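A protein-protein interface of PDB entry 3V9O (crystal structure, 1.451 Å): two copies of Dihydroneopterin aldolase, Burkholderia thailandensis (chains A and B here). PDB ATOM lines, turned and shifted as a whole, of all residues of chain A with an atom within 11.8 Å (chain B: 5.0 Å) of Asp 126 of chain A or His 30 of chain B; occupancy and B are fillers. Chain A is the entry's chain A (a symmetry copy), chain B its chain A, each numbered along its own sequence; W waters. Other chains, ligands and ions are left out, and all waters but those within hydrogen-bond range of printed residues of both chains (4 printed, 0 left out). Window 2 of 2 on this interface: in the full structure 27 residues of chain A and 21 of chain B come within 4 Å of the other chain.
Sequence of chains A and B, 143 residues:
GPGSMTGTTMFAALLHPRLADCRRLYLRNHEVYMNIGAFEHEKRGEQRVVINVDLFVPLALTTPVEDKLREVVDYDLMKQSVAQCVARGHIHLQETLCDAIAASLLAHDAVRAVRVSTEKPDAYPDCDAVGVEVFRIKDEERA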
ATOM      1  N   LYS A 120      -3.465 -30.140  21.949  1.00  0.00           N
ATOM      2  CA  LYS A 120      -2.374 -30.185  22.908  1.00  0.00           C
ATOM      3  C   LYS A 120      -2.929 -30.077  24.302  1.00  0.00           C
ATOM      4  O   LYS A 120      -3.335 -28.974  24.759  1.00  0.00           O
ATOM      5  CB  LYS A 120      -1.436 -28.988  22.680  1.00  0.00           C
ATOM      6  CG  LYS A 120      -0.559 -29.161  21.510  1.00  0.00           C
ATOM      7  CD  LYS A 120       0.310 -27.839  21.367  1.00  0.00           C
ATOM      8  CE  LYS A 120       1.069 -27.795  20.165  1.00  0.00           C
ATOM      9  NZ  LYS A 120       2.061 -26.601  20.304  1.00  0.00           N
ATOM     10  N   PRO A 121      -2.946 -31.189  25.038  1.00  0.00           N
ATOM     11  CA  PRO A 121      -3.434 -31.123  26.436  1.00  0.00           C
ATOM     12  C   PRO A 121      -2.601 -30.230  27.318  1.00  0.00           C
ATOM     13  O   PRO A 121      -3.159 -29.767  28.342  1.00  0.00           O
ATOM     14  CB  PRO A 121      -3.376 -32.570  26.938  1.00  0.00           C
ATOM     15  CG  PRO A 121      -2.389 -33.268  25.933  1.00  0.00           C
ATOM     16  CD  PRO A 121      -2.622 -32.576  24.636  1.00  0.00           C
ATOM     17  N   ASP A 122      -1.334 -30.030  26.993  1.00  0.00           N
ATOM     18  CA  ASP A 122      -0.433 -29.283  27.918  1.00  0.00           C
ATOM     19  C   ASP A 122      -0.153 -27.890  27.425  1.00  0.00           C
ATOM     20  O   ASP A 122       0.790 -27.255  28.001  1.00  0.00           O
ATOM     21  CB  ASP A 122       0.854 -30.055  28.176  1.00  0.00           C
ATOM     22  CG  ASP A 122       0.575 -31.436  28.678  1.00  0.00           C
ATOM     23  OD1 ASP A 122      -0.326 -31.588  29.528  1.00  0.00           O
ATOM     24  OD2 ASP A 122       1.192 -32.383  28.172  1.00  0.00           O
ATOM     25  N   ALA A 123      -0.898 -27.356  26.479  1.00  0.00           N
ATOM     26  CA  ALA A 123      -0.637 -25.980  26.050  1.00  0.00           C
ATOM     27  C   ALA A 123      -0.739 -24.968  27.183  1.00  0.00           C
ATOM     28  O   ALA A 123       0.103 -24.046  27.276  1.00  0.00           O
ATOM     29  CB  ALA A 123      -1.590 -25.597  24.904  1.00  0.00           C
ATOM     30  N   TYR A 124      -1.736 -25.119  28.047  1.00  0.00           N
ATOM     31  CA  TYR A 124      -1.951 -24.136  29.100  1.00  0.00           C
ATOM     32  C   TYR A 124      -2.237 -24.854  30.409  1.00  0.00           C
ATOM     33  O   TYR A 124      -3.076 -25.791  30.414  1.00  0.00           O
ATOM     34  CB  TYR A 124      -3.197 -23.275  28.787  1.00  0.00           C
ATOM     35  CG  TYR A 124      -3.271 -22.668  27.391  1.00  0.00           C
ATOM     36  CD1 TYR A 124      -2.305 -21.735  26.957  1.00  0.00           C
ATOM     37  CD2 TYR A 124      -4.282 -23.042  26.516  1.00  0.00           C
ATOM     38  CE1 TYR A 124      -2.363 -21.209  25.677  1.00  0.00           C
ATOM     39  CE2 TYR A 124      -4.340 -22.487  25.212  1.00  0.00           C
ATOM     40  CZ  TYR A 124      -3.416 -21.580  24.843  1.00  0.00           C
ATOM     41  OH  TYR A 124      -3.602 -21.046  23.569  1.00  0.00           O
ATOM     42  N   PRO A 125      -1.689 -24.390  31.528  1.00  0.00           N
ATOM     43  CA  PRO A 125      -1.926 -25.083  32.825  1.00  0.00           C
ATOM     44  C   PRO A 125      -3.400 -25.067  33.274  1.00  0.00           C
ATOM     45  O   PRO A 125      -3.819 -25.987  34.015  1.00  0.00           O
ATOM     46  CB  PRO A 125      -1.103 -24.265  33.806  1.00  0.00           C
ATOM     47  CG  PRO A 125       0.038 -23.709  32.944  1.00  0.00           C
ATOM     48  CD  PRO A 125      -0.701 -23.301  31.652  1.00  0.00           C
ATOM     49  N   ASP A 126      -4.166 -24.058  32.831  1.00  0.00           N
ATOM     50  CA  ASP A 126      -5.555 -23.875  33.313  1.00  0.00           C
ATOM     51  C   ASP A 126      -6.584 -24.247  32.248  1.00  0.00           C
ATOM     52  O   ASP A 126      -7.743 -23.832  32.358  1.00  0.00           O
ATOM     53  CB  ASP A 126      -5.749 -22.408  33.788  1.00  0.00           C
ATOM     54  CG  ASP A 126      -5.419 -21.397  32.709  1.00  0.00           C
ATOM     55  OD1 ASP A 126      -4.974 -21.773  31.593  1.00  0.00           O
ATOM     56  OD2 ASP A 126      -5.540 -20.185  33.036  1.00  0.00           O
ATOM     57  N   CYS A 127      -6.221 -25.068  31.270  1.00  0.00           N
ATOM     58  CA  CYS A 127      -7.151 -25.567  30.259  1.00  0.00           C
ATOM     59  C   CYS A 127      -6.913 -27.032  30.021  1.00  0.00           C
ATOM     60  O   CYS A 127      -5.734 -27.503  30.103  1.00  0.00           O
ATOM     61  CB  CYS A 127      -6.961 -24.845  28.930  1.00  0.00           C
ATOM     62  SG  CYS A 127      -7.138 -23.048  28.960  1.00  0.00           S
ATOM     63  N   ASP A 128      -7.944 -27.788  29.692  1.00  0.00           N
ATOM     64  CA  ASP A 128      -7.767 -29.207  29.375  1.00  0.00           C
ATOM     65  C   ASP A 128      -7.053 -29.390  28.037  1.00  0.00           C
ATOM     66  O   ASP A 128      -6.297 -30.370  27.877  1.00  0.00           O
ATOM     67  CB  ASP A 128      -9.079 -29.979  29.367  1.00  0.00           C
ATOM     68  CG  ASP A 128      -9.590 -30.282  30.754  1.00  0.00           C
ATOM     69  OD1 ASP A 128      -8.940 -29.948  31.777  1.00  0.00           O
ATOM     70  OD2 ASP A 128     -10.713 -30.841  30.845  1.00  0.00           O
ATOM     71  N   ALA A 129      -7.346 -28.562  27.036  1.00  0.00           N
ATOM     72  CA  ALA A 129      -6.675 -28.678  25.719  1.00  0.00           C
ATOM     73  C   ALA A 129      -6.923 -27.485  24.845  1.00  0.00           C
ATOM     74  O   ALA A 129      -7.917 -26.754  25.089  1.00  0.00           O
ATOM     75  CB  ALA A 129      -7.183 -29.928  24.975  1.00  0.00           C
ATOM     76  N   VAL A 130      -6.080 -27.264  23.853  1.00  0.00           N
ATOM     77  CA  VAL A 130      -6.411 -26.353  22.765  1.00  0.00           C
ATOM     78  C   VAL A 130      -6.127 -27.147  21.492  1.00  0.00           C
ATOM     79  O   VAL A 130      -5.103 -27.837  21.406  1.00  0.00           O
ATOM     80  CB  VAL A 130      -5.567 -25.028  22.862  1.00  0.00           C
ATOM     81  CG1 VAL A 130      -4.082 -25.275  22.634  1.00  0.00           C
ATOM     82  CG2 VAL A 130      -6.101 -23.958  21.889  1.00  0.00           C
ATOM     83  N   GLY A 131      -7.011 -26.991  20.527  1.00  0.00           N
ATOM     84  CA  GLY A 131      -6.916 -27.816  19.326  1.00  0.00           C
ATOM     85  C   GLY A 131      -7.494 -27.163  18.112  1.00  0.00           C
ATOM     86  O   GLY A 131      -8.001 -26.048  18.082  1.00  0.00           O
ATOM     87  N   LEU B  27     -10.919 -24.324  22.528  1.00  0.00           N
ATOM     88  CA  LEU B  27     -10.325 -24.289  23.871  1.00  0.00           C
ATOM     89  C   LEU B  27     -11.271 -25.063  24.771  1.00  0.00           C
ATOM     90  O   LEU B  27     -12.481 -24.733  24.917  1.00  0.00           O
ATOM     91  CB  LEU B  27     -10.274 -22.811  24.322  1.00  0.00           C
ATOM     92  CG  LEU B  27      -9.429 -22.635  25.584  1.00  0.00           C
ATOM     93  CD1 LEU B  27      -7.956 -22.942  25.363  1.00  0.00           C
ATOM     94  CD2 LEU B  27      -9.631 -21.157  26.077  1.00  0.00           C
ATOM     95  N   ARG B  28     -10.786 -26.173  25.342  1.00  0.00           N
ATOM     96  CA  ARG B  28     -11.619 -27.042  26.160  1.00  0.00           C
ATOM     97  C   ARG B  28     -11.351 -26.845  27.638  1.00  0.00           C
ATOM     98  O   ARG B  28     -10.197 -26.958  28.087  1.00  0.00           O
ATOM     99  CB  ARG B  28     -11.420 -28.542  25.815  1.00  0.00           C
ATOM    100  CG  ARG B  28     -12.390 -29.423  26.560  1.00  0.00           C
ATOM    101  CD  ARG B  28     -12.615 -30.835  26.011  1.00  0.00           C
ATOM    102  NE  ARG B  28     -11.415 -31.641  26.169  1.00  0.00           N
ATOM    103  CZ  ARG B  28     -10.594 -32.008  25.165  1.00  0.00           C
ATOM    104  NH1 ARG B  28     -10.856 -31.717  23.918  1.00  0.00           N
ATOM    105  NH2 ARG B  28      -9.540 -32.722  25.479  1.00  0.00           N
ATOM    106  N   ASN B  29     -12.442 -26.586  28.363  1.00  0.00           N
ATOM    107  CA  ASN B  29     -12.432 -26.487  29.860  1.00  0.00           C
ATOM    108  C   ASN B  29     -11.330 -25.563  30.370  1.00  0.00           C
ATOM    109  O   ASN B  29     -10.423 -26.020  31.116  1.00  0.00           O
ATOM    110  CB  ASN B  29     -12.389 -27.841  30.522  1.00  0.00           C
ATOM    111  CG  ASN B  29     -13.610 -28.671  30.181  1.00  0.00           C
ATOM    112  OD1 ASN B  29     -14.727 -28.108  30.004  1.00  0.00           O
ATOM    113  ND2 ASN B  29     -13.449 -29.993  30.125  1.00  0.00           N
ATOM    114  N   HIS B  30     -11.412 -24.277  30.000  1.00  0.00           N
ATOM    115  CA  HIS B  30     -10.564 -23.278  30.594  1.00  0.00           C
ATOM    116  C   HIS B  30     -11.205 -22.878  31.911  1.00  0.00           C
ATOM    117  O   HIS B  30     -12.286 -22.322  31.939  1.00  0.00           O
ATOM    118  CB  HIS B  30     -10.470 -22.078  29.639  1.00  0.00           C
ATOM    119  CG  HIS B  30      -9.720 -20.927  30.188  1.00  0.00           C
ATOM    120  ND1 HIS B  30      -8.726 -21.055  31.121  1.00  0.00           N
ATOM    121  CD2 HIS B  30      -9.770 -19.606  29.876  1.00  0.00           C
ATOM    122  CE1 HIS B  30      -8.218 -19.862  31.405  1.00  0.00           C
ATOM    123  NE2 HIS B  30      -8.855 -18.968  30.677  1.00  0.00           N
ATOM    124  N   GLU B  31     -10.528 -23.142  33.009  1.00  0.00           N
ATOM    125  CA  GLU B  31     -11.039 -22.755  34.332  1.00  0.00           C
ATOM    126  C   GLU B  31     -10.441 -21.411  34.755  1.00  0.00           C
ATOM    127  O   GLU B  31      -9.269 -21.119  34.574  1.00  0.00           O
ATOM    128  CB  GLU B  31     -10.739 -23.824  35.373  1.00  0.00           C
ATOM    129  CG  GLU B  31      -9.321 -24.001  35.772  1.00  0.00           C
ATOM    130  CD  GLU B  31      -9.152 -24.797  37.022  1.00  0.00           C
ATOM    131  OE1 GLU B  31     -10.104 -25.468  37.499  1.00  0.00           O
ATOM    132  OE2 GLU B  31      -8.035 -24.767  37.567  1.00  0.00           O
ATOM    133  N   VAL B  32     -11.334 -20.632  35.385  1.00  0.00           N
ATOM    134  CA  VAL B  32     -10.928 -19.398  36.035  1.00  0.00           C
ATOM    135  C   VAL B  32     -11.603 -19.328  37.392  1.00  0.00           C
ATOM    136  O   VAL B  32     -12.637 -19.979  37.651  1.00  0.00           O
ATOM    137  CB  VAL B  32     -11.314 -18.147  35.201  1.00  0.00           C
ATOM    138  CG1 VAL B  32     -10.619 -18.143  33.817  1.00  0.00           C
ATOM    139  CG2 VAL B  32     -12.824 -17.979  35.051  1.00  0.00           C
ATOM    140  N   VAL B  49     -15.267 -21.017  37.498  1.00  0.00           N
ATOM    141  CA  VAL B  49     -16.089 -20.946  36.276  1.00  0.00           C
ATOM    142  C   VAL B  49     -15.327 -21.678  35.209  1.00  0.00           C
ATOM    143  O   VAL B  49     -14.095 -21.486  35.055  1.00  0.00           O
ATOM    144  CB  VAL B  49     -16.356 -19.470  35.875  1.00  0.00           C
ATOM    145  CG1 VAL B  49     -17.183 -19.410  34.554  1.00  0.00           C
ATOM    146  CG2 VAL B  49     -17.091 -18.725  36.994  1.00  0.00           C
ATOM    147  N   VAL B  50     -16.006 -22.553  34.435  1.00  0.00           N
ATOM    148  CA  VAL B  50     -15.333 -23.335  33.369  1.00  0.00           C
ATOM    149  C   VAL B  50     -15.882 -22.842  32.025  1.00  0.00           C
ATOM    150  O   VAL B  50     -17.134 -22.746  31.826  1.00  0.00           O
ATOM    151  CB  VAL B  50     -15.581 -24.824  33.568  1.00  0.00           C
ATOM    152  CG1 VAL B  50     -14.996 -25.626  32.405  1.00  0.00           C
ATOM    153  CG2 VAL B  50     -14.964 -25.300  34.923  1.00  0.00           C
ATOM    154  N   ILE B  51     -14.964 -22.522  31.122  1.00  0.00           N
ATOM    155  CA  ILE B  51     -15.298 -21.831  29.853  1.00  0.00           C
ATOM    156  C   ILE B  51     -14.847 -22.690  28.686  1.00  0.00           C
ATOM    157  O   ILE B  51     -13.743 -23.241  28.701  1.00  0.00           O
ATOM    158  CB  ILE B  51     -14.604 -20.475  29.827  1.00  0.00           C
ATOM    159  CG1 ILE B  51     -15.166 -19.664  30.991  1.00  0.00           C
ATOM    160  CG2 ILE B  51     -14.914 -19.751  28.473  1.00  0.00           C
ATOM    161  CD1 ILE B  51     -14.421 -18.468  31.352  1.00  0.00           C
ATOM    162  N   LYS B  79      -7.837 -17.802  24.899  1.00  0.00           N
ATOM    163  CA  LYS B  79      -7.532 -17.624  26.306  1.00  0.00           C
ATOM    164  C   LYS B  79      -7.317 -16.136  26.601  1.00  0.00           C
ATOM    165  O   LYS B  79      -7.783 -15.661  27.651  1.00  0.00           O
ATOM    166  CB  LYS B  79      -6.315 -18.497  26.694  1.00  0.00           C
ATOM    167  CG  LYS B  79      -6.012 -18.512  28.188  1.00  0.00           C
ATOM    168  CD  LYS B  79      -4.876 -19.440  28.637  1.00  0.00           C
ATOM    169  CE  LYS B  79      -4.467 -18.991  30.088  1.00  0.00           C
ATOM    170  NZ  LYS B  79      -3.434 -19.748  30.740  1.00  0.00           N
ATOM    171  N   VAL B  82     -10.733 -14.443  27.020  1.00  0.00           N
ATOM    172  CA  VAL B  82     -11.362 -14.788  28.305  1.00  0.00           C
ATOM    173  C   VAL B  82     -10.664 -14.008  29.400  1.00  0.00           C
ATOM    174  O   VAL B  82     -11.337 -13.377  30.242  1.00  0.00           O
ATOM    175  CB  VAL B  82     -11.223 -16.283  28.563  1.00  0.00           C
ATOM    176  CG1 VAL B  82     -11.722 -16.590  29.995  1.00  0.00           C
ATOM    177  CG2 VAL B  82     -12.078 -17.027  27.539  1.00  0.00           C
HETATM  178  O   HOH W   1     -11.371 -32.775  28.972  1.00  0.00           O
HETATM  179  O   HOH W   2      -7.247 -19.380  35.018  1.00  0.00           O
HETATM  180  O   HOH W   3      -6.451 -19.999  23.652  1.00  0.00           O
HETATM  181  O   HOH W   4      -7.168 -32.984  27.678  1.00  0.00           O
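No position is printed for both chains. Of the 14 pairs that touch across the chains among the printed residues, none has its exchanged pair printed and touching as well.
Of the printed residues of chain B, Asp 126 of chain A touches Asn 29, His 30, Glu 31 and Lys 79. His 30 of chain B touches just these residues of chain A: Asp 126 (3.2 Å) and Cys 127 (3.3 Å). Printed residues of chain A within 4 Å of Leu 27 of chain B: Tyr 124 (3.6 Å), Cys 127 (3.7 Å) and Ala 129 (3.7 Å). Of chain A, only Asp 126, Cys 127 and Asp 128 come within 4 Å of Asn 29 of chain B. Glu 31 of chain B touches just one residue of chain A: Asp 126 (2.9 Å). Val 50 of chain B touches none of the printed residues of chain A. No residue of chain A comes within 4 Å of Ile 51 of chain B. Of the printed residues of chain A, Lys 79 of chain B touches Tyr 124 (3.8 Å) and Asp 126 (2.7 Å). Printed residues of chain A within 4 Å of Arg 28 of chain B: Cys 127, Asp 128 and Ala 129. Printed residues of chain B within 4 Å of Ala 129 of chain A: Leu 27 and Arg 28. Printed residues of chain B within 4 Å of Tyr 124 of chain A: Leu 27 (3.6 Å) and Lys 79 (3.8 Å). Printed residues of chain B within 4 Å of Asp 128 of chain A: Arg 28 (2.9 Å) and Asn 29 (3.0 Å). Pro 121 of chain A touches none of the printed residues of chain B. The nearest printed residue of chain B that does not touch Asp 126 of chain A is Val 32 of chain B (5.5 Å). The nearest residue of chain A that does not touch His 30 of chain B is Asp 128 of chain A (4.9 Å).
O of Ala 129 of chain A sits at hydrogen-bond distance from N of Arg 28 of chain B (2.9 Å). The backbone carbonyl oxygen (O) of Asp 126 of chain A sits at hydrogen-bond distance from a ring nitrogen (ND1) of His 30 of chain B, at 3.2 Å. NZ of Lys 79 of chain B lies within salt-bridge range of OD1 of Asp 126 of chain A, at 2.7 Å. The side-chain carboxylate of Asp 128 of chain A is in hydrogen-bond range of the side-chain amide nitrogen of Asn 29 of chain B (3.0 Å). The backbone NH (N) of Asp 128 of chain A sits at hydrogen-bond distance from the backbone carbonyl oxygen (O) of Arg 28 of chain B, 2.9 Å away. A ring nitrogen (ND1) of His 30 of chain B sits at hydrogen-bond distance from the side-chain sulfur of Cys 127 of chain A (3.3 Å). The backbone carbonyl oxygen (O) of Asp 126 of chain A lies within hydrogen-bond range of the backbone NH (N) of Glu 31 of chain B.
The backbone carbonyl oxygen (O) of His 30 of chain B sits at hydrogen-bond distance from the backbone NH (N) of Ile 51 of chain B, at 2.8 Å. OD1 of Asp 126 of chain A sits close to SG of Cys 127 of chain A (3.6 Å).
CD1 of Leu 27 of chain B touches CE2 of Tyr 124 of chain A (3.6 Å). Tyr 124 of chain A touches Lys 79 of chain B. Asp 126 of chain A touches Asn 29 of chain B (O to O, 3.7 Å). SG of Cys 127 of chain A touches CD1 of Leu 27 of chain B, at 3.7 Å. Cys 127 of chain A touches Arg 28 of chain B. O of Asn 29 of chain B touches CA of Cys 127 of chain A, at 3.4 Å. Ala 129 of chain A touches Leu 27 of chain B.
Of the 12 printed residues of chain A, 5 touch a printed residue of chain B. Hydrophobic or aromatic side chains of chain A within 4 Å of the printed part of chain B: Tyr 124 and Ala 129. Printed residues of chain B that touch a printed residue of chain A: Leu 27, Arg 28, Asn 29, His 30, Glu 31 and Lys 79.
Water W2 lies within hydrogen-bond range of the backbone carbonyl oxygen of Glu 31 of chain B and the side-chain carboxylate of Asp 126 of chain A. Water W4 bridges O of Asp 128 of chain A (2.8 Å) and NH2 of Arg 28 of chain B (3.2 Å). Water W1 lies within hydrogen-bond range of OD2 of Asp 128 of chain A and NE of Arg 28 of chain B. Water W3 bridges the backbone NH (N) of Lys 79 of chain B (2.9 Å) and the side-chain hydroxyl (OH) of Tyr 124 of chain A (3.0 Å).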
